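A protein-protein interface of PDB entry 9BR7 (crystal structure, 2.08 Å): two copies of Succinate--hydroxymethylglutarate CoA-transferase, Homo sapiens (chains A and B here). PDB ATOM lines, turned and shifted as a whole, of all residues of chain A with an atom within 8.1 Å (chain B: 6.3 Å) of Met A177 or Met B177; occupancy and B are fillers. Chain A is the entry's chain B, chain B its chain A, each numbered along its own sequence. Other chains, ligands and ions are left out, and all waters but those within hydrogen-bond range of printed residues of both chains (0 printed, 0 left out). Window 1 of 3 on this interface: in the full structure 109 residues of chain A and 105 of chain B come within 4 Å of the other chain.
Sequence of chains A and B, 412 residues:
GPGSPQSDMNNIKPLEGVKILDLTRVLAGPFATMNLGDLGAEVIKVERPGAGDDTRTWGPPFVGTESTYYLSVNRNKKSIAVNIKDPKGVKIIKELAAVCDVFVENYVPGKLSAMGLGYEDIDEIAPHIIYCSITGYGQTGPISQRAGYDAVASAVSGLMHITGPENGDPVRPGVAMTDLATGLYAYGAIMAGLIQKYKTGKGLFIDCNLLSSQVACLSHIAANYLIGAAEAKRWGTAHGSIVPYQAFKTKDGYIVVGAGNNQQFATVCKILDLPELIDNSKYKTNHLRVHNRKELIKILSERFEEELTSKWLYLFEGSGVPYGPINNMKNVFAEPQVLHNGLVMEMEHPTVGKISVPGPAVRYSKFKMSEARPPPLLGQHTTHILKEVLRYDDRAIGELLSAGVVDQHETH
OD2 of Asp B150 is in hydrogen-bond range of N of Met B177 (3.4 Å). The side-chain hydroxyl (OG1) of Thr B178 lies within hydrogen-bond range of the side-chain amide oxygen (OE1) of Gln B214, 2.6 Å away. O of Ser A154 lies within hydrogen-bond range of N of Leu A159 (3.2 Å). OG1 of Thr A163 sits at hydrogen-bond distance from O of Leu A159 (2.7 Å). The side-chain hydroxyl of Thr A178 is in hydrogen-bond range of the side-chain amide oxygen of Gln A214, at 2.9 Å. O of Ser A213 is in hydrogen-bond range of SG of Cys A217, at 3.4 Å.
Printed residues of chain B within 4 Å of Leu A159: Gly B174. Of the printed residues of chain B, Met A177 touches Met B177 (3.98 Å) and Gln B214 (3.9 Å). Ala A181 touches none of the printed residues of chain B. Printed residues of chain A within 4 Å of Pro B173: Thr A163 (3.7 Å). Ala B176 touches none of the printed residues of chain A. Met B177 touches three residues of chain A. Printed residues of chain A within 4 Å of Leu B180: Cys A217. The nearest residue of chain B that does not touch Met A177 is Cys B217 (4.1 Å). The nearest printed residue of chain A that does not touch Val B175 is Leu A159 (4.1 Å).
Met B177 touches its own counterpart, Met A177. Met A177 touches Gln B214, and with the chains exchanged Gln A214 touches Met B177. Leu A180 touches Cys B217, and with the chains exchanged Cys A217 touches Leu B180. Cys A217 touches Met B177, but with the chains exchanged Met A177 does not touch Cys B217 (4.1 Å). Positions printed for both chains: 150, 159, 173, 174, 175, 176, 177, 178, 179, 180, 181, 182, 214 and 217. Of the 13 pairs that touch across the chains among the printed residues, 7 have their exchanged pair printed and touching as well.
Among the printed residues, pairs that only touch across the chains: Leu A180 with Cys B217, Cys A217 with Leu B180, Val A175 with Cys B217, Leu A184 with Ala B181, Cys A217 with Val B175, Thr A163 with Pro B173, Met A177 with Gln B214, Leu A218 with Val B175, Cys A217 with Met B177, Leu A159 with Gly B174 and Met A177 with Met B177.
Hydrophobic or aromatic side chains of chain B that line the printed part of chain A: Val B175, Met B177 and Leu B180. Of the 27 printed residues of chain A, 9 touch a printed residue of chain B. Printed residues of chain A that touch a printed residue of chain B: Leu A159, Thr A163, Val A175, Met A177, Leu A180, Leu A184, Gln A214, Cys A217 and Leu A218. Hydrophobic or aromatic side chains of chain A within 4 Å of the printed part of chain B: Leu A159, Val A175, Met A177, Leu A180 and Leu A184. Along chain A the printed residues that touch a printed residue of chain B span positions 159 to 218. Among the printed residues, no Asp or Glu carboxylate lies within 4 Å of a Lys or Arg side-chain nitrogen of the other chain.
N of Gly B174 is in hydrogen-bond range of OG1 of Thr A163, 2.7 Å away. SD of Met B177 is in hydrogen-bond range of NE2 of Gln A214.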
ATOM      1  N   LEU A  27       9.342 -24.106  -1.017  1.00  0.00           N
ATOM      2  CA  LEU A  27       8.526 -23.901   0.176  1.00  0.00           C
ATOM      3  C   LEU A  27       7.388 -24.909   0.328  1.00  0.00           C
ATOM      4  O   LEU A  27       7.273 -25.563   1.369  1.00  0.00           O
ATOM      5  CB  LEU A  27       7.964 -22.477   0.181  1.00  0.00           C
ATOM      6  CG  LEU A  27       7.022 -22.124   1.330  1.00  0.00           C
ATOM      7  CD1 LEU A  27       7.736 -22.281   2.663  1.00  0.00           C
ATOM      8  CD2 LEU A  27       6.504 -20.709   1.166  1.00  0.00           C
ATOM      9  N   PHE A  31       7.704 -27.519   3.262  1.00  0.00           N
ATOM     10  CA  PHE A  31       6.833 -27.257   4.404  1.00  0.00           C
ATOM     11  C   PHE A  31       5.996 -28.482   4.748  1.00  0.00           C
ATOM     12  O   PHE A  31       5.796 -28.797   5.928  1.00  0.00           O
ATOM     13  CB  PHE A  31       5.940 -26.049   4.118  1.00  0.00           C
ATOM     14  CG  PHE A  31       5.138 -25.589   5.303  1.00  0.00           C
ATOM     15  CD1 PHE A  31       5.763 -25.001   6.392  1.00  0.00           C
ATOM     16  CD2 PHE A  31       3.759 -25.723   5.319  1.00  0.00           C
ATOM     17  CE1 PHE A  31       5.028 -24.570   7.483  1.00  0.00           C
ATOM     18  CE2 PHE A  31       3.018 -25.291   6.406  1.00  0.00           C
ATOM     19  CZ  PHE A  31       3.653 -24.714   7.490  1.00  0.00           C
ATOM     20  N   ASP A 150       4.102 -18.940  -6.096  1.00  0.00           N
ATOM     21  CA  ASP A 150       3.043 -18.492  -5.197  1.00  0.00           C
ATOM     22  C   ASP A 150       2.392 -17.209  -5.702  1.00  0.00           C
ATOM     23  O   ASP A 150       1.161 -17.102  -5.751  1.00  0.00           O
ATOM     24  CB  ASP A 150       3.591 -18.303  -3.783  1.00  0.00           C
ATOM     25  CG  ASP A 150       2.554 -17.729  -2.832  1.00  0.00           C
ATOM     26  OD1 ASP A 150       2.235 -16.529  -2.954  1.00  0.00           O
ATOM     27  OD2 ASP A 150       2.042 -18.480  -1.976  1.00  0.00           O
ATOM     28  N   ALA A 151       3.206 -16.217  -6.078  1.00  0.00           N
ATOM     29  CA  ALA A 151       2.651 -14.938  -6.511  1.00  0.00           C
ATOM     30  C   ALA A 151       1.816 -15.100  -7.774  1.00  0.00           C
ATOM     31  O   ALA A 151       0.777 -14.449  -7.929  1.00  0.00           O
ATOM     32  CB  ALA A 151       3.772 -13.923  -6.736  1.00  0.00           C
ATOM     33  N   SER A 154      -1.563 -16.996  -6.794  1.00  0.00           N
ATOM     34  CA  SER A 154      -2.521 -16.113  -6.137  1.00  0.00           C
ATOM     35  C   SER A 154      -3.117 -15.107  -7.112  1.00  0.00           C
ATOM     36  O   SER A 154      -4.234 -14.622  -6.895  1.00  0.00           O
ATOM     37  CB  SER A 154      -1.855 -15.392  -4.966  1.00  0.00           C
ATOM     38  OG  SER A 154      -1.100 -14.283  -5.417  1.00  0.00           O
ATOM     39  N   LEU A 159      -7.229 -14.768  -5.749  1.00  0.00           N
ATOM     40  CA  LEU A 159      -6.979 -14.246  -4.409  1.00  0.00           C
ATOM     41  C   LEU A 159      -6.527 -12.793  -4.460  1.00  0.00           C
ATOM     42  O   LEU A 159      -6.986 -11.965  -3.664  1.00  0.00           O
ATOM     43  CB  LEU A 159      -5.935 -15.106  -3.697  1.00  0.00           C
ATOM     44  CG  LEU A 159      -5.528 -14.656  -2.293  1.00  0.00           C
ATOM     45  CD1 LEU A 159      -6.745 -14.559  -1.384  1.00  0.00           C
ATOM     46  CD2 LEU A 159      -4.481 -15.588  -1.700  1.00  0.00           C
ATOM     47  N   THR A 163      -8.059  -9.090  -2.762  1.00  0.00           N
ATOM     48  CA  THR A 163      -7.200  -8.678  -1.659  1.00  0.00           C
ATOM     49  C   THR A 163      -6.615  -7.312  -1.979  1.00  0.00           C
ATOM     50  O   THR A 163      -5.978  -7.135  -3.024  1.00  0.00           O
ATOM     51  CB  THR A 163      -6.085  -9.699  -1.416  1.00  0.00           C
ATOM     52  OG1 THR A 163      -6.659 -10.981  -1.133  1.00  0.00           O
ATOM     53  CG2 THR A 163      -5.213  -9.271  -0.245  1.00  0.00           C
ATOM     54  N   ARG A 172      -0.850  -8.801  -2.570  1.00  0.00           N
ATOM     55  CA  ARG A 172      -0.622 -10.208  -2.293  1.00  0.00           C
ATOM     56  C   ARG A 172      -0.434 -10.415  -0.794  1.00  0.00           C
ATOM     57  O   ARG A 172       0.047  -9.515  -0.097  1.00  0.00           O
ATOM     58  CB  ARG A 172       0.607 -10.746  -3.033  1.00  0.00           C
ATOM     59  CG  ARG A 172       1.924 -10.283  -2.449  1.00  0.00           C
ATOM     60  CD  ARG A 172       3.100 -10.928  -3.161  1.00  0.00           C
ATOM     61  NE  ARG A 172       4.362 -10.490  -2.583  1.00  0.00           N
ATOM     62  CZ  ARG A 172       4.925 -11.048  -1.520  1.00  0.00           C
ATOM     63  NH1 ARG A 172       4.375 -12.086  -0.913  1.00  0.00           N
ATOM     64  NH2 ARG A 172       6.062 -10.545  -1.048  1.00  0.00           N
ATOM     65  N   PRO A 173      -0.796 -11.580  -0.262  1.00  0.00           N
ATOM     66  CA  PRO A 173      -0.515 -11.851   1.152  1.00  0.00           C
ATOM     67  C   PRO A 173       0.967 -11.689   1.459  1.00  0.00           C
ATOM     68  O   PRO A 173       1.830 -11.991   0.630  1.00  0.00           O
ATOM     69  CB  PRO A 173      -0.979 -13.300   1.335  1.00  0.00           C
ATOM     70  CG  PRO A 173      -1.999 -13.504   0.260  1.00  0.00           C
ATOM     71  CD  PRO A 173      -1.533 -12.680  -0.905  1.00  0.00           C
ATOM     72  N   GLY A 174       1.256 -11.193   2.665  1.00  0.00           N
ATOM     73  CA  GLY A 174       2.635 -10.943   3.051  1.00  0.00           C
ATOM     74  C   GLY A 174       3.525 -12.166   2.941  1.00  0.00           C
ATOM     75  O   GLY A 174       4.710 -12.048   2.619  1.00  0.00           O
ATOM     76  N   VAL A 175       2.977 -13.348   3.213  1.00  0.00           N
ATOM     77  CA  VAL A 175       3.704 -14.601   3.073  1.00  0.00           C
ATOM     78  C   VAL A 175       3.001 -15.447   2.018  1.00  0.00           C
ATOM     79  O   VAL A 175       1.850 -15.198   1.651  1.00  0.00           O
ATOM     80  CB  VAL A 175       3.816 -15.367   4.408  1.00  0.00           C
ATOM     81  CG1 VAL A 175       2.492 -16.032   4.757  1.00  0.00           C
ATOM     82  CG2 VAL A 175       4.944 -16.390   4.347  1.00  0.00           C
ATOM     83  N   ALA A 176       3.715 -16.464   1.532  1.00  0.00           N
ATOM     84  CA  ALA A 176       3.224 -17.310   0.442  1.00  0.00           C
ATOM     85  C   ALA A 176       2.170 -18.282   0.975  1.00  0.00           C
ATOM     86  O   ALA A 176       2.384 -19.489   1.100  1.00  0.00           O
ATOM     87  CB  ALA A 176       4.382 -18.047  -0.219  1.00  0.00           C
ATOM     88  N   MET A 177       0.996 -17.722   1.286  1.00  0.00           N
ATOM     89  CA  MET A 177      -0.088 -18.532   1.835  1.00  0.00           C
ATOM     90  C   MET A 177      -0.586 -19.569   0.837  1.00  0.00           C
ATOM     91  O   MET A 177      -1.069 -20.632   1.242  1.00  0.00           O
ATOM     92  CB  MET A 177      -1.242 -17.641   2.293  1.00  0.00           C
ATOM     93  CG  MET A 177      -0.949 -16.859   3.561  1.00  0.00           C
ATOM     94  SD  MET A 177      -0.483 -17.932   4.934  1.00  0.00           S
ATOM     95  CE  MET A 177      -2.022 -18.802   5.227  1.00  0.00           C
ATOM     96  N   THR A 178      -0.503 -19.279  -0.462  1.00  0.00           N
ATOM     97  CA  THR A 178      -0.910 -20.274  -1.450  1.00  0.00           C
ATOM     98  C   THR A 178       0.011 -21.488  -1.417  1.00  0.00           C
ATOM     99  O   THR A 178      -0.462 -22.632  -1.439  1.00  0.00           O
ATOM    100  CB  THR A 178      -0.940 -19.653  -2.846  1.00  0.00           C
ATOM    101  OG1 THR A 178      -1.827 -18.526  -2.848  1.00  0.00           O
ATOM    102  CG2 THR A 178      -1.418 -20.669  -3.870  1.00  0.00           C
ATOM    103  N   ASP A 179       1.326 -21.263  -1.356  1.00  0.00           N
ATOM    104  CA  ASP A 179       2.264 -22.371  -1.205  1.00  0.00           C
ATOM    105  C   ASP A 179       2.013 -23.127   0.094  1.00  0.00           C
ATOM    106  O   ASP A 179       1.959 -24.363   0.109  1.00  0.00           O
ATOM    107  CB  ASP A 179       3.703 -21.857  -1.254  1.00  0.00           C
ATOM    108  CG  ASP A 179       4.256 -21.793  -2.666  1.00  0.00           C
ATOM    109  OD1 ASP A 179       3.576 -22.273  -3.599  1.00  0.00           O
ATOM    110  OD2 ASP A 179       5.377 -21.270  -2.843  1.00  0.00           O
ATOM    111  N   LEU A 180       1.864 -22.397   1.202  1.00  0.00           N
ATOM    112  CA  LEU A 180       1.707 -23.049   2.499  1.00  0.00           C
ATOM    113  C   LEU A 180       0.401 -23.828   2.576  1.00  0.00           C
ATOM    114  O   LEU A 180       0.374 -24.953   3.088  1.00  0.00           O
ATOM    115  CB  LEU A 180       1.788 -22.010   3.618  1.00  0.00           C
ATOM    116  CG  LEU A 180       3.133 -21.289   3.717  1.00  0.00           C
ATOM    117  CD1 LEU A 180       3.049 -20.093   4.653  1.00  0.00           C
ATOM    118  CD2 LEU A 180       4.205 -22.260   4.186  1.00  0.00           C
ATOM    119  N   ALA A 181      -0.692 -23.252   2.071  1.00  0.00           N
ATOM    120  CA  ALA A 181      -1.955 -23.983   2.027  1.00  0.00           C
ATOM    121  C   ALA A 181      -1.802 -25.275   1.236  1.00  0.00           C
ATOM    122  O   ALA A 181      -2.265 -26.339   1.662  1.00  0.00           O
ATOM    123  CB  ALA A 181      -3.050 -23.103   1.425  1.00  0.00           C
ATOM    124  N   THR A 182      -1.159 -25.198   0.068  1.00  0.00           N
ATOM    125  CA  THR A 182      -0.897 -26.402  -0.709  1.00  0.00           C
ATOM    126  C   THR A 182      -0.067 -27.397   0.091  1.00  0.00           C
ATOM    127  O   THR A 182      -0.337 -28.604   0.071  1.00  0.00           O
ATOM    128  CB  THR A 182      -0.193 -26.041  -2.018  1.00  0.00           C
ATOM    129  OG1 THR A 182      -0.987 -25.095  -2.745  1.00  0.00           O
ATOM    130  CG2 THR A 182       0.009 -27.284  -2.872  1.00  0.00           C
ATOM    131  N   GLY A 183       0.949 -26.909   0.806  1.00  0.00           N
ATOM    132  CA  GLY A 183       1.737 -27.796   1.645  1.00  0.00           C
ATOM    133  C   GLY A 183       0.906 -28.491   2.708  1.00  0.00           C
ATOM    134  O   GLY A 183       1.097 -29.680   2.977  1.00  0.00           O
ATOM    135  N   LEU A 184      -0.026 -27.762   3.328  1.00  0.00           N
ATOM    136  CA  LEU A 184      -0.877 -28.370   4.345  1.00  0.00           C
ATOM    137  C   LEU A 184      -1.846 -29.371   3.727  1.00  0.00           C
ATOM    138  O   LEU A 184      -2.105 -30.432   4.309  1.00  0.00           O
ATOM    139  CB  LEU A 184      -1.633 -27.289   5.118  1.00  0.00           C
ATOM    140  CG  LEU A 184      -0.774 -26.371   5.991  1.00  0.00           C
ATOM    141  CD1 LEU A 184      -1.614 -25.244   6.565  1.00  0.00           C
ATOM    142  CD2 LEU A 184      -0.104 -27.161   7.106  1.00  0.00           C
ATOM    143  N   TYR A 185      -2.391 -29.055   2.551  1.00  0.00           N
ATOM    144  CA  TYR A 185      -3.199 -30.030   1.826  1.00  0.00           C
ATOM    145  C   TYR A 185      -2.420 -31.324   1.616  1.00  0.00           C
ATOM    146  O   TYR A 185      -2.931 -32.421   1.866  1.00  0.00           O
ATOM    147  CB  TYR A 185      -3.642 -29.454   0.479  1.00  0.00           C
ATOM    148  CG  TYR A 185      -5.002 -28.788   0.475  1.00  0.00           C
ATOM    149  CD1 TYR A 185      -6.166 -29.534   0.613  1.00  0.00           C
ATOM    150  CD2 TYR A 185      -5.124 -27.414   0.307  1.00  0.00           C
ATOM    151  CE1 TYR A 185      -7.413 -28.927   0.600  1.00  0.00           C
ATOM    152  CE2 TYR A 185      -6.362 -26.800   0.290  1.00  0.00           C
ATOM    153  CZ  TYR A 185      -7.502 -27.560   0.437  1.00  0.00           C
ATOM    154  OH  TYR A 185      -8.735 -26.947   0.420  1.00  0.00           O
ATOM    155  N   LEU A 210      -0.984 -25.531  -6.645  1.00  0.00           N
ATOM    156  CA  LEU A 210      -1.289 -24.224  -6.071  1.00  0.00           C
ATOM    157  C   LEU A 210      -2.650 -23.714  -6.530  1.00  0.00           C
ATOM    158  O   LEU A 210      -3.412 -23.157  -5.731  1.00  0.00           O
ATOM    159  CB  LEU A 210      -0.193 -23.227  -6.448  1.00  0.00           C
ATOM    160  CG  LEU A 210       1.238 -23.606  -6.065  1.00  0.00           C
ATOM    161  CD1 LEU A 210       2.203 -22.484  -6.414  1.00  0.00           C
ATOM    162  CD2 LEU A 210       1.323 -23.949  -4.587  1.00  0.00           C
ATOM    163  N   SER A 213      -5.583 -25.569  -4.748  1.00  0.00           N
ATOM    164  CA  SER A 213      -5.647 -25.216  -3.334  1.00  0.00           C
ATOM    165  C   SER A 213      -6.281 -23.845  -3.134  1.00  0.00           C
ATOM    166  O   SER A 213      -7.164 -23.673  -2.284  1.00  0.00           O
ATOM    167  CB  SER A 213      -4.248 -25.257  -2.719  1.00  0.00           C
ATOM    168  OG  SER A 213      -3.697 -26.561  -2.790  1.00  0.00           O
ATOM    169  N   GLN A 214      -5.843 -22.852  -3.911  1.00  0.00           N
ATOM    170  CA  GLN A 214      -6.309 -21.487  -3.683  1.00  0.00           C
ATOM    171  C   GLN A 214      -7.756 -21.308  -4.126  1.00  0.00           C
ATOM    172  O   GLN A 214      -8.527 -20.601  -3.468  1.00  0.00           O
ATOM    173  CB  GLN A 214      -5.401 -20.490  -4.399  1.00  0.00           C
ATOM    174  CG  GLN A 214      -5.618 -19.060  -3.947  1.00  0.00           C
ATOM    175  CD  GLN A 214      -5.545 -18.922  -2.438  1.00  0.00           C
ATOM    176  OE1 GLN A 214      -4.470 -19.014  -1.846  1.00  0.00           O
ATOM    177  NE2 GLN A 214      -6.695 -18.714  -1.807  1.00  0.00           N
ATOM    178  N   ALA A 216     -10.061 -23.572  -4.070  1.00  0.00           N
ATOM    179  CA  ALA A 216     -10.867 -24.181  -3.017  1.00  0.00           C
ATOM    180  C   ALA A 216     -11.013 -23.245  -1.824  1.00  0.00           C
ATOM    181  O   ALA A 216     -12.074 -23.193  -1.192  1.00  0.00           O
ATOM    182  CB  ALA A 216     -10.248 -25.511  -2.586  1.00  0.00           C
ATOM    183  N   CYS A 217      -9.957 -22.493  -1.502  1.00  0.00           N
ATOM    184  CA  CYS A 217     -10.014 -21.571  -0.374  1.00  0.00           C
ATOM    185  C   CYS A 217     -10.944 -20.394  -0.633  1.00  0.00           C
ATOM    186  O   CYS A 217     -11.318 -19.696   0.314  1.00  0.00           O
ATOM    187  CB  CYS A 217      -8.613 -21.059  -0.037  1.00  0.00           C
ATOM    188  SG  CYS A 217      -7.558 -22.268   0.786  1.00  0.00           S
ATOM    189  N   LEU A 218     -11.309 -20.144  -1.892  1.00  0.00           N
ATOM    190  CA  LEU A 218     -12.270 -19.085  -2.179  1.00  0.00           C
ATOM    191  C   LEU A 218     -13.627 -19.383  -1.552  1.00  0.00           C
ATOM    192  O   LEU A 218     -14.335 -18.457  -1.139  1.00  0.00           O
ATOM    193  CB  LEU A 218     -12.403 -18.897  -3.690  1.00  0.00           C
ATOM    194  CG  LEU A 218     -11.155 -18.357  -4.396  1.00  0.00           C
ATOM    195  CD1 LEU A 218     -11.427 -18.116  -5.875  1.00  0.00           C
ATOM    196  CD2 LEU A 218     -10.637 -17.094  -3.723  1.00  0.00           C
ATOM    197  N   ASP B 150     -10.660 -14.791  12.466  1.00  0.00           N
ATOM    198  CA  ASP B 150      -9.596 -14.776  11.466  1.00  0.00           C
ATOM    199  C   ASP B 150      -8.944 -13.402  11.378  1.00  0.00           C
ATOM    200  O   ASP B 150      -7.714 -13.284  11.414  1.00  0.00           O
ATOM    201  CB  ASP B 150     -10.143 -15.206  10.103  1.00  0.00           C
ATOM    202  CG  ASP B 150      -9.100 -15.112   8.999  1.00  0.00           C
ATOM    203  OD1 ASP B 150      -8.692 -13.982   8.652  1.00  0.00           O
ATOM    204  OD2 ASP B 150      -8.674 -16.168   8.490  1.00  0.00           O
ATOM    205  N   LEU B 159       0.428 -11.287  10.288  1.00  0.00           N
ATOM    206  CA  LEU B 159       0.141 -11.367   8.858  1.00  0.00           C
ATOM    207  C   LEU B 159      -0.313 -10.024   8.297  1.00  0.00           C
ATOM    208  O   LEU B 159       0.138  -9.614   7.221  1.00  0.00           O
ATOM    209  CB  LEU B 159      -0.916 -12.437   8.590  1.00  0.00           C
ATOM    210  CG  LEU B 159      -1.328 -12.582   7.122  1.00  0.00           C
ATOM    211  CD1 LEU B 159      -0.111 -12.871   6.247  1.00  0.00           C
ATOM    212  CD2 LEU B 159      -2.383 -13.666   6.959  1.00  0.00           C
ATOM    213  N   PRO B 173      -6.222 -10.772   3.849  1.00  0.00           N
ATOM    214  CA  PRO B 173      -6.449 -11.629   2.682  1.00  0.00           C
ATOM    215  C   PRO B 173      -7.920 -11.618   2.295  1.00  0.00           C
ATOM    216  O   PRO B 173      -8.806 -11.510   3.144  1.00  0.00           O
ATOM    217  CB  PRO B 173      -6.004 -13.015   3.162  1.00  0.00           C
ATOM    218  CG  PRO B 173      -5.045 -12.736   4.275  1.00  0.00           C
ATOM    219  CD  PRO B 173      -5.552 -11.491   4.946  1.00  0.00           C
ATOM    220  N   GLY B 174      -8.176 -11.719   0.990  1.00  0.00           N
ATOM    221  CA  GLY B 174      -9.550 -11.685   0.519  1.00  0.00           C
ATOM    222  C   GLY B 174     -10.425 -12.720   1.197  1.00  0.00           C
ATOM    223  O   GLY B 174     -11.615 -12.483   1.421  1.00  0.00           O
ATOM    224  N   VAL B 175      -9.856 -13.878   1.522  1.00  0.00           N
ATOM    225  CA  VAL B 175     -10.548 -14.919   2.265  1.00  0.00           C
ATOM    226  C   VAL B 175      -9.804 -15.153   3.574  1.00  0.00           C
ATOM    227  O   VAL B 175      -8.648 -14.757   3.743  1.00  0.00           O
ATOM    228  CB  VAL B 175     -10.669 -16.227   1.460  1.00  0.00           C
ATOM    229  CG1 VAL B 175     -11.560 -16.017   0.248  1.00  0.00           C
ATOM    230  CG2 VAL B 175      -9.292 -16.711   1.035  1.00  0.00           C
ATOM    231  N   ALA B 176     -10.488 -15.818   4.505  1.00  0.00           N
ATOM    232  CA  ALA B 176      -9.959 -16.058   5.849  1.00  0.00           C
ATOM    233  C   ALA B 176      -8.916 -17.177   5.791  1.00  0.00           C
ATOM    234  O   ALA B 176      -9.132 -18.309   6.226  1.00  0.00           O
ATOM    235  CB  ALA B 176     -11.088 -16.389   6.813  1.00  0.00           C
ATOM    236  N   MET B 177      -7.749 -16.827   5.241  1.00  0.00           N
ATOM    237  CA  MET B 177      -6.688 -17.813   5.063  1.00  0.00           C
ATOM    238  C   MET B 177      -6.181 -18.356   6.393  1.00  0.00           C
ATOM    239  O   MET B 177      -5.739 -19.509   6.460  1.00  0.00           O
ATOM    240  CB  MET B 177      -5.535 -17.203   4.263  1.00  0.00           C
ATOM    241  CG  MET B 177      -5.842 -16.997   2.786  1.00  0.00           C
ATOM    242  SD  MET B 177      -6.335 -18.521   1.957  1.00  0.00           S
ATOM    243  CE  MET B 177      -4.805 -19.447   2.029  1.00  0.00           C
ATOM    244  N   THR B 178      -6.223 -17.552   7.458  1.00  0.00           N
ATOM    245  CA  THR B 178      -5.813 -18.063   8.763  1.00  0.00           C
ATOM    246  C   THR B 178      -6.768 -19.147   9.249  1.00  0.00           C
ATOM    247  O   THR B 178      -6.331 -20.190   9.750  1.00  0.00           O
ATOM    248  CB  THR B 178      -5.723 -16.927   9.780  1.00  0.00           C
ATOM    249  OG1 THR B 178      -4.813 -15.928   9.303  1.00  0.00           O
ATOM    250  CG2 THR B 178      -5.223 -17.453  11.118  1.00  0.00           C
ATOM    251  N   ASP B 179      -8.076 -18.919   9.104  1.00  0.00           N
ATOM    252  CA  ASP B 179      -9.051 -19.953   9.436  1.00  0.00           C
ATOM    253  C   ASP B 179      -8.826 -21.200   8.590  1.00  0.00           C
ATOM    254  O   ASP B 179      -8.813 -22.323   9.107  1.00  0.00           O
ATOM    255  CB  ASP B 179     -10.470 -19.419   9.231  1.00  0.00           C
ATOM    256  CG  ASP B 179     -11.018 -18.714  10.459  1.00  0.00           C
ATOM    257  OD1 ASP B 179     -10.361 -18.755  11.522  1.00  0.00           O
ATOM    258  OD2 ASP B 179     -12.107 -18.111  10.357  1.00  0.00           O
ATOM    259  N   LEU B 180      -8.647 -21.019   7.278  1.00  0.00           N
ATOM    260  CA  LEU B 180      -8.500 -22.163   6.387  1.00  0.00           C
ATOM    261  C   LEU B 180      -7.212 -22.926   6.668  1.00  0.00           C
ATOM    262  O   LEU B 180      -7.210 -24.162   6.687  1.00  0.00           O
ATOM    263  CB  LEU B 180      -8.550 -21.699   4.931  1.00  0.00           C
ATOM    264  CG  LEU B 180      -9.870 -21.049   4.512  1.00  0.00           C
ATOM    265  CD1 LEU B 180      -9.746 -20.375   3.152  1.00  0.00           C
ATOM    266  CD2 LEU B 180     -10.979 -22.087   4.499  1.00  0.00           C
ATOM    267  N   ALA B 181      -6.106 -22.210   6.885  1.00  0.00           N
ATOM    268  CA  ALA B 181      -4.857 -22.875   7.243  1.00  0.00           C
ATOM    269  C   ALA B 181      -5.020 -23.691   8.519  1.00  0.00           C
ATOM    270  O   ALA B 181      -4.577 -24.844   8.594  1.00  0.00           O
ATOM    271  CB  ALA B 181      -3.737 -21.845   7.395  1.00  0.00           C
ATOM    272  N   THR B 182      -5.649 -23.104   9.540  1.00  0.00           N
ATOM    273  CA  THR B 182      -5.905 -23.841  10.773  1.00  0.00           C
ATOM    274  C   THR B 182      -6.747 -25.081  10.502  1.00  0.00           C
ATOM    275  O   THR B 182      -6.479 -26.158  11.050  1.00  0.00           O
ATOM    276  CB  THR B 182      -6.595 -22.938  11.796  1.00  0.00           C
ATOM    277  OG1 THR B 182      -5.792 -21.773  12.024  1.00  0.00           O
ATOM    278  CG2 THR B 182      -6.784 -23.677  13.113  1.00  0.00           C
ATOM    279  N   GLN B 214      -0.988 -19.350  12.166  1.00  0.00           N
ATOM    280  CA  GLN B 214      -0.514 -18.218  11.377  1.00  0.00           C
ATOM    281  C   GLN B 214       0.946 -17.897  11.676  1.00  0.00           C
ATOM    282  O   GLN B 214       1.710 -17.559  10.764  1.00  0.00           O
ATOM    283  CB  GLN B 214      -1.392 -16.993  11.627  1.00  0.00           C
ATOM    284  CG  GLN B 214      -1.169 -15.873  10.625  1.00  0.00           C
ATOM    285  CD  GLN B 214      -1.276 -16.345   9.190  1.00  0.00           C
ATOM    286  OE1 GLN B 214      -2.367 -16.641   8.701  1.00  0.00           O
ATOM    287  NE2 GLN B 214      -0.139 -16.421   8.504  1.00  0.00           N
ATOM    288  N   CYS B 217       3.056 -20.258   9.852  1.00  0.00           N
ATOM    289  CA  CYS B 217       3.090 -19.950   8.428  1.00  0.00           C
ATOM    290  C   CYS B 217       3.986 -18.760   8.112  1.00  0.00           C
ATOM    291  O   CYS B 217       4.383 -18.595   6.954  1.00  0.00           O
ATOM    292  CB  CYS B 217       1.675 -19.695   7.908  1.00  0.00           C
ATOM    293  SG  CYS B 217       0.678 -21.193   7.729  1.00  0.00           S
